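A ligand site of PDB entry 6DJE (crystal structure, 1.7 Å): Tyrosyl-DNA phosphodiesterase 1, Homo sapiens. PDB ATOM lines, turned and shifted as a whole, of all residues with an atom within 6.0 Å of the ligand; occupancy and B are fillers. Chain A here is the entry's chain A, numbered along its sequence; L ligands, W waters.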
ATOM      1  N   ASN A  56     -36.263   9.804  -8.955  1.00  0.00           N
ATOM      2  CA  ASN A  56     -34.916  10.328  -8.714  1.00  0.00           C
ATOM      3  C   ASN A  56     -34.906  11.192  -7.462  1.00  0.00           C
ATOM      4  O   ASN A  56     -35.915  11.323  -6.765  1.00  0.00           O
ATOM      5  CB  ASN A  56     -34.392  11.104  -9.935  1.00  0.00           C
ATOM      6  CG  ASN A  56     -32.906  10.883 -10.146  1.00  0.00           C
ATOM      7  OD1 ASN A  56     -32.098  11.355  -9.357  1.00  0.00           O
ATOM      8  ND2 ASN A  56     -32.542  10.109 -11.173  1.00  0.00           N
ATOM      9  N   TYR A  57     -33.739  11.772  -7.187  1.00  0.00           N
ATOM     10  CA  TYR A  57     -33.510  12.636  -6.045  1.00  0.00           C
ATOM     11  C   TYR A  57     -33.488  14.094  -6.502  1.00  0.00           C
ATOM     12  O   TYR A  57     -34.275  14.912  -6.021  1.00  0.00           O
ATOM     13  CB  TYR A  57     -32.194  12.241  -5.356  1.00  0.00           C
ATOM     14  CG  TYR A  57     -31.782  13.216  -4.277  1.00  0.00           C
ATOM     15  CD1 TYR A  57     -32.544  13.361  -3.132  1.00  0.00           C
ATOM     16  CD2 TYR A  57     -30.637  13.987  -4.420  1.00  0.00           C
ATOM     17  CE1 TYR A  57     -32.176  14.267  -2.148  1.00  0.00           C
ATOM     18  CE2 TYR A  57     -30.272  14.890  -3.455  1.00  0.00           C
ATOM     19  CZ  TYR A  57     -31.030  15.020  -2.319  1.00  0.00           C
ATOM     20  OH  TYR A  57     -30.639  15.934  -1.359  1.00  0.00           O
ATOM     21  N   HIS A 116     -34.068   8.463  -2.644  1.00  0.00           N
ATOM     22  CA  HIS A 116     -32.778   8.333  -3.336  1.00  0.00           C
ATOM     23  C   HIS A 116     -32.841   7.411  -4.550  1.00  0.00           C
ATOM     24  O   HIS A 116     -31.904   7.414  -5.364  1.00  0.00           O
ATOM     25  CB  HIS A 116     -31.714   7.811  -2.379  1.00  0.00           C
ATOM     26  CG  HIS A 116     -31.094   8.883  -1.536  1.00  0.00           C
ATOM     27  ND1 HIS A 116     -30.490   8.630  -0.322  1.00  0.00           N
ATOM     28  CD2 HIS A 116     -30.987  10.222  -1.738  1.00  0.00           C
ATOM     29  CE1 HIS A 116     -30.029   9.756   0.184  1.00  0.00           C
ATOM     30  NE2 HIS A 116     -30.327  10.740  -0.652  1.00  0.00           N
ATOM     31  N   LYS A 118     -33.155   5.788  -8.046  1.00  0.00           N
ATOM     32  CA  LYS A 118     -32.992   6.253  -9.424  1.00  0.00           C
ATOM     33  C   LYS A 118     -33.493   5.169 -10.361  1.00  0.00           C
ATOM     34  O   LYS A 118     -32.859   4.111 -10.506  1.00  0.00           O
ATOM     35  CB  LYS A 118     -31.540   6.610  -9.760  1.00  0.00           C
ATOM     36  CG  LYS A 118     -30.745   7.216  -8.635  1.00  0.00           C
ATOM     37  CD  LYS A 118     -31.244   8.582  -8.295  1.00  0.00           C
ATOM     38  CE  LYS A 118     -30.106   9.420  -7.692  1.00  0.00           C
ATOM     39  NZ  LYS A 118     -29.692   8.868  -6.382  1.00  0.00           N
ATOM     40  N   THR A 134     -27.825   5.011 -11.130  1.00  0.00           N
ATOM     41  CA  THR A 134     -27.287   5.725  -9.971  1.00  0.00           C
ATOM     42  C   THR A 134     -27.197   7.235 -10.169  1.00  0.00           C
ATOM     43  O   THR A 134     -26.758   7.926  -9.239  1.00  0.00           O
ATOM     44  CB  THR A 134     -25.879   5.202  -9.599  1.00  0.00           C
ATOM     45  OG1 THR A 134     -24.957   5.417 -10.672  1.00  0.00           O
ATOM     46  CG2 THR A 134     -25.909   3.721  -9.311  1.00  0.00           C
ATOM     47  N   SER A 135     -27.615   7.781 -11.314  1.00  0.00           N
ATOM     48  CA  SER A 135     -27.389   9.190 -11.635  1.00  0.00           C
ATOM     49  C   SER A 135     -28.604  10.042 -11.311  1.00  0.00           C
ATOM     50  O   SER A 135     -29.746   9.659 -11.592  1.00  0.00           O
ATOM     51  CB  SER A 135     -27.073   9.384 -13.129  1.00  0.00           C
ATOM     52  OG  SER A 135     -25.936   8.644 -13.524  1.00  0.00           O
ATOM     53  N   ASN A 136     -28.343  11.226 -10.749  1.00  0.00           N
ATOM     54  CA  ASN A 136     -29.359  12.285 -10.679  1.00  0.00           C
ATOM     55  C   ASN A 136     -29.659  12.813 -12.092  1.00  0.00           C
ATOM     56  O   ASN A 136     -28.874  12.642 -13.020  1.00  0.00           O
ATOM     57  CB  ASN A 136     -28.881  13.425  -9.779  1.00  0.00           C
ATOM     58  CG  ASN A 136     -28.842  13.020  -8.314  1.00  0.00           C
ATOM     59  OD1 ASN A 136     -29.878  12.980  -7.646  1.00  0.00           O
ATOM     60  ND2 ASN A 136     -27.647  12.698  -7.807  1.00  0.00           N
ATOM     61  N   ASP A 141     -24.214  14.990 -13.406  1.00  0.00           N
ATOM     62  CA  ASP A 141     -24.154  13.583 -13.019  1.00  0.00           C
ATOM     63  C   ASP A 141     -23.894  12.654 -14.191  1.00  0.00           C
ATOM     64  O   ASP A 141     -23.502  11.506 -13.983  1.00  0.00           O
ATOM     65  CB  ASP A 141     -25.449  13.162 -12.304  1.00  0.00           C
ATOM     66  CG  ASP A 141     -25.310  13.241 -10.801  1.00  0.00           C
ATOM     67  OD1 ASP A 141     -24.659  14.200 -10.321  1.00  0.00           O
ATOM     68  OD2 ASP A 141     -25.790  12.324 -10.093  1.00  0.00           O
ATOM     69  N   SER A 252     -20.532   6.749  -2.308  1.00  0.00           N
ATOM     70  CA  SER A 252     -20.199   8.165  -2.500  1.00  0.00           C
ATOM     71  C   SER A 252     -20.535   9.035  -1.288  1.00  0.00           C
ATOM     72  O   SER A 252     -20.286  10.251  -1.343  1.00  0.00           O
ATOM     73  CB  SER A 252     -20.894   8.708  -3.753  1.00  0.00           C
ATOM     74  OG  SER A 252     -22.296   8.618  -3.663  1.00  0.00           O
ATOM     75  N   GLY A 311     -18.705  18.198  -4.405  1.00  0.00           N
ATOM     76  CA  GLY A 311     -20.072  18.596  -4.127  1.00  0.00           C
ATOM     77  C   GLY A 311     -21.040  17.431  -4.164  1.00  0.00           C
ATOM     78  O   GLY A 311     -22.141  17.543  -3.615  1.00  0.00           O
ATOM     79  N   SER A 312     -20.653  16.310  -4.787  1.00  0.00           N
ATOM     80  CA  SER A 312     -21.495  15.118  -4.876  1.00  0.00           C
ATOM     81  C   SER A 312     -20.949  13.966  -4.012  1.00  0.00           C
ATOM     82  O   SER A 312     -21.312  12.800  -4.226  1.00  0.00           O
ATOM     83  CB  SER A 312     -21.634  14.656  -6.323  1.00  0.00           C
ATOM     84  OG  SER A 312     -22.279  15.632  -7.114  1.00  0.00           O
ATOM     85  N   LEU A 313     -20.097  14.284  -3.049  1.00  0.00           N
ATOM     86  CA  LEU A 313     -19.543  13.325  -2.096  1.00  0.00           C
ATOM     87  C   LEU A 313     -19.737  13.935  -0.714  1.00  0.00           C
ATOM     88  O   LEU A 313     -18.785  14.413  -0.088  1.00  0.00           O
ATOM     89  CB  LEU A 313     -18.064  13.044  -2.387  1.00  0.00           C
ATOM     90  CG  LEU A 313     -17.674  12.438  -3.754  1.00  0.00           C
ATOM     91  CD1 LEU A 313     -16.186  12.669  -4.093  1.00  0.00           C
ATOM     92  CD2 LEU A 313     -17.980  10.935  -3.806  1.00  0.00           C
ATOM     93  N   PRO A 314     -20.986  13.952  -0.212  1.00  0.00           N
ATOM     94  CA  PRO A 314     -21.351  14.816   0.923  1.00  0.00           C
ATOM     95  C   PRO A 314     -21.072  14.213   2.310  1.00  0.00           C
ATOM     96  O   PRO A 314     -21.972  14.032   3.129  1.00  0.00           O
ATOM     97  CB  PRO A 314     -22.852  15.034   0.697  1.00  0.00           C
ATOM     98  CG  PRO A 314     -23.315  13.794   0.017  1.00  0.00           C
ATOM     99  CD  PRO A 314     -22.163  13.319  -0.845  1.00  0.00           C
ATOM    100  N   HIS A 346     -20.096   8.168  -8.474  1.00  0.00           N
ATOM    101  CA  HIS A 346     -21.411   8.331  -7.876  1.00  0.00           C
ATOM    102  C   HIS A 346     -22.197   7.028  -7.922  1.00  0.00           C
ATOM    103  O   HIS A 346     -23.255   6.912  -7.288  1.00  0.00           O
ATOM    104  CB  HIS A 346     -22.138   9.491  -8.576  1.00  0.00           C
ATOM    105  CG  HIS A 346     -23.398   9.913  -7.896  1.00  0.00           C
ATOM    106  ND1 HIS A 346     -24.634   9.411  -8.237  1.00  0.00           N
ATOM    107  CD2 HIS A 346     -23.622  10.793  -6.884  1.00  0.00           C
ATOM    108  CE1 HIS A 346     -25.572   9.977  -7.480  1.00  0.00           C
ATOM    109  NE2 HIS A 346     -24.975  10.805  -6.644  1.00  0.00           N
ATOM    110  N   LYS A 348     -22.792   3.251  -6.618  1.00  0.00           N
ATOM    111  CA  LYS A 348     -22.551   2.521  -5.378  1.00  0.00           C
ATOM    112  C   LYS A 348     -22.619   1.031  -5.697  1.00  0.00           C
ATOM    113  O   LYS A 348     -23.536   0.597  -6.407  1.00  0.00           O
ATOM    114  CB  LYS A 348     -23.577   2.847  -4.272  1.00  0.00           C
ATOM    115  CG  LYS A 348     -23.590   4.307  -3.835  1.00  0.00           C
ATOM    116  CD  LYS A 348     -24.551   5.101  -4.719  1.00  0.00           C
ATOM    117  CE  LYS A 348     -24.766   6.500  -4.175  1.00  0.00           C
ATOM    118  NZ  LYS A 348     -24.928   7.459  -5.280  1.00  0.00           N
ATOM    119  N   SER A 367     -28.496   2.534  -5.408  1.00  0.00           N
ATOM    120  CA  SER A 367     -28.433   3.913  -4.957  1.00  0.00           C
ATOM    121  C   SER A 367     -27.979   4.032  -3.511  1.00  0.00           C
ATOM    122  O   SER A 367     -27.648   5.140  -3.068  1.00  0.00           O
ATOM    123  CB  SER A 367     -29.803   4.584  -5.134  1.00  0.00           C
ATOM    124  OG  SER A 367     -30.761   3.917  -4.337  1.00  0.00           O
ATOM    125  N   ASN A 369     -26.008   4.333  -0.243  1.00  0.00           N
ATOM    126  CA  ASN A 369     -24.701   4.658   0.314  1.00  0.00           C
ATOM    127  C   ASN A 369     -24.480   3.896   1.623  1.00  0.00           C
ATOM    128  O   ASN A 369     -25.326   3.104   2.049  1.00  0.00           O
ATOM    129  CB  ASN A 369     -24.588   6.166   0.542  1.00  0.00           C
ATOM    130  CG  ASN A 369     -24.170   6.899  -0.709  1.00  0.00           C
ATOM    131  OD1 ASN A 369     -23.213   6.500  -1.375  1.00  0.00           O
ATOM    132  ND2 ASN A 369     -24.890   7.972  -1.048  1.00  0.00           N
ATOM    133  N   GLU A 391     -34.484   3.548  -1.515  1.00  0.00           N
ATOM    134  CA  GLU A 391     -33.290   3.165  -2.285  1.00  0.00           C
ATOM    135  C   GLU A 391     -33.660   1.996  -3.173  1.00  0.00           C
ATOM    136  O   GLU A 391     -34.619   1.267  -2.907  1.00  0.00           O
ATOM    137  CB  GLU A 391     -32.109   2.726  -1.387  1.00  0.00           C
ATOM    138  CG  GLU A 391     -31.817   3.630  -0.198  1.00  0.00           C
ATOM    139  CD  GLU A 391     -30.997   4.860  -0.574  1.00  0.00           C
ATOM    140  OE1 GLU A 391     -30.862   5.773   0.275  1.00  0.00           O
ATOM    141  OE2 GLU A 391     -30.487   4.923  -1.722  1.00  0.00           O
ATOM    142  N   TRP A 443     -16.607  17.214   2.604  1.00  0.00           N
ATOM    143  CA  TRP A 443     -16.991  18.221   1.621  1.00  0.00           C
ATOM    144  C   TRP A 443     -17.115  19.626   2.204  1.00  0.00           C
ATOM    145  O   TRP A 443     -17.085  20.586   1.443  1.00  0.00           O
ATOM    146  CB  TRP A 443     -18.298  17.864   0.917  1.00  0.00           C
ATOM    147  CG  TRP A 443     -19.561  17.990   1.739  1.00  0.00           C
ATOM    148  CD1 TRP A 443     -19.685  17.866   3.095  1.00  0.00           C
ATOM    149  CD2 TRP A 443     -20.871  18.238   1.238  1.00  0.00           C
ATOM    150  NE1 TRP A 443     -20.999  18.034   3.467  1.00  0.00           N
ATOM    151  CE2 TRP A 443     -21.747  18.265   2.346  1.00  0.00           C
ATOM    152  CE3 TRP A 443     -21.400  18.448  -0.040  1.00  0.00           C
ATOM    153  CZ2 TRP A 443     -23.119  18.497   2.213  1.00  0.00           C
ATOM    154  CZ3 TRP A 443     -22.762  18.676  -0.173  1.00  0.00           C
ATOM    155  CH2 TRP A 443     -23.598  18.692   0.952  1.00  0.00           C
HETATM  156  C1  LIG L   1     -28.259  12.522  -2.332  1.00  0.00           C
HETATM  157  C2  LIG L   1     -26.905  14.374  -1.920  1.00  0.00           C
HETATM  158  C3  LIG L   1     -26.720  15.059   1.415  1.00  0.00           C
HETATM  159  C4  LIG L   1     -27.381  15.707   0.202  1.00  0.00           C
HETATM  160  C5  LIG L   1     -27.595  17.205   0.453  1.00  0.00           C
HETATM  161  C6  LIG L   1     -26.581  15.462  -1.084  1.00  0.00           C
HETATM  162  C7  LIG L   1     -25.534  16.315  -1.423  1.00  0.00           C
HETATM  163  C8  LIG L   1     -24.805  16.091  -2.591  1.00  0.00           C
HETATM  164  C9  LIG L   1     -25.128  15.005  -3.418  1.00  0.00           C
HETATM  165  C10 LIG L   1     -26.187  14.148  -3.066  1.00  0.00           C
HETATM  166  C11 LIG L   1     -26.520  13.066  -3.892  1.00  0.00           C
HETATM  167  C12 LIG L   1     -27.573  12.247  -3.506  1.00  0.00           C
HETATM  168  C13 LIG L   1     -28.002  11.028  -4.327  1.00  0.00           C
HETATM  169  N1  LIG L   1     -27.918  13.554  -1.570  1.00  0.00           N
HETATM  170  O1  LIG L   1     -25.898  12.875  -4.898  1.00  0.00           O
HETATM  171  O2  LIG L   1     -27.825  11.003  -5.572  1.00  0.00           O
HETATM  172  O3  LIG L   1     -28.531  10.037  -3.744  1.00  0.00           O
HETATM  173  O   HOH W   1     -25.446   9.600  -3.546  1.00  0.00           O
HETATM  174  O   HOH W   2     -24.734  14.557  -7.541  1.00  0.00           O
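Water W1 lies within hydrogen-bond range of the side-chain amino group (NZ) of Lys 348 (2.8 Å), the side-chain amide nitrogen (ND2) of Asn 369 (3.0 Å), an oxygen (O3) of the ligand (3.1 Å), the side-chain hydroxyl (OG) of Ser 252 (3.3 Å) and a ring nitrogen (NE2) of His 346 (3.4 Å). Water W2 lies within hydrogen-bond range of the side-chain hydroxyl of Ser 312 (2.7 Å), the side-chain carboxylate of Asp 141 (2.8 Å), an oxygen (O1) of the ligand (3.3 Å) and the side-chain amide nitrogen of Asn 136 (3.5 Å).
An oxygen (O2) of the ligand lies within salt-bridge range of the side-chain amino group (NZ) of Lys 118. An oxygen (O2) of the ligand lies within hydrogen-bond range of the side-chain amide nitrogen (ND2) of Asn 136 (2.8 Å). NE2 of His 346 is in hydrogen-bond range of O1 of the ligand, 2.9 Å away.
O of Thr 134 lies within hydrogen-bond range of ND1 of His 346 (2.8 Å). OE1 of Glu 391 sits at hydrogen-bond distance from ND1 of His 116, 2.9 Å away. OD1 of Asn 136 sits close to OD1 of Asn 56. N of Asn 136 lies within hydrogen-bond range of OD2 of Asp 141, 2.9 Å away. ND2 of Asn 136 sits close to NE2 of His 346, 3.5 Å away. O of His 346 sits at hydrogen-bond distance from NZ of Lys 348 (2.7 Å). The side-chain amino group of Lys 118 is in hydrogen-bond range of the backbone carbonyl oxygen of His 116.
Residues that only touch the ligand: His 116, Gly 311, Tyr 57, Pro 314, Trp 443 and Ser 312. Hydrophobic or aromatic side chains within 4 Å of the ligand: Tyr 57, His 116, Pro 314, His 346 and Trp 443. Within 4 Å of the ligand: Tyr 57, His 116, Lys 118, Asn 136, Gly 311, Ser 312, Pro 314, His 346 and Trp 443.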
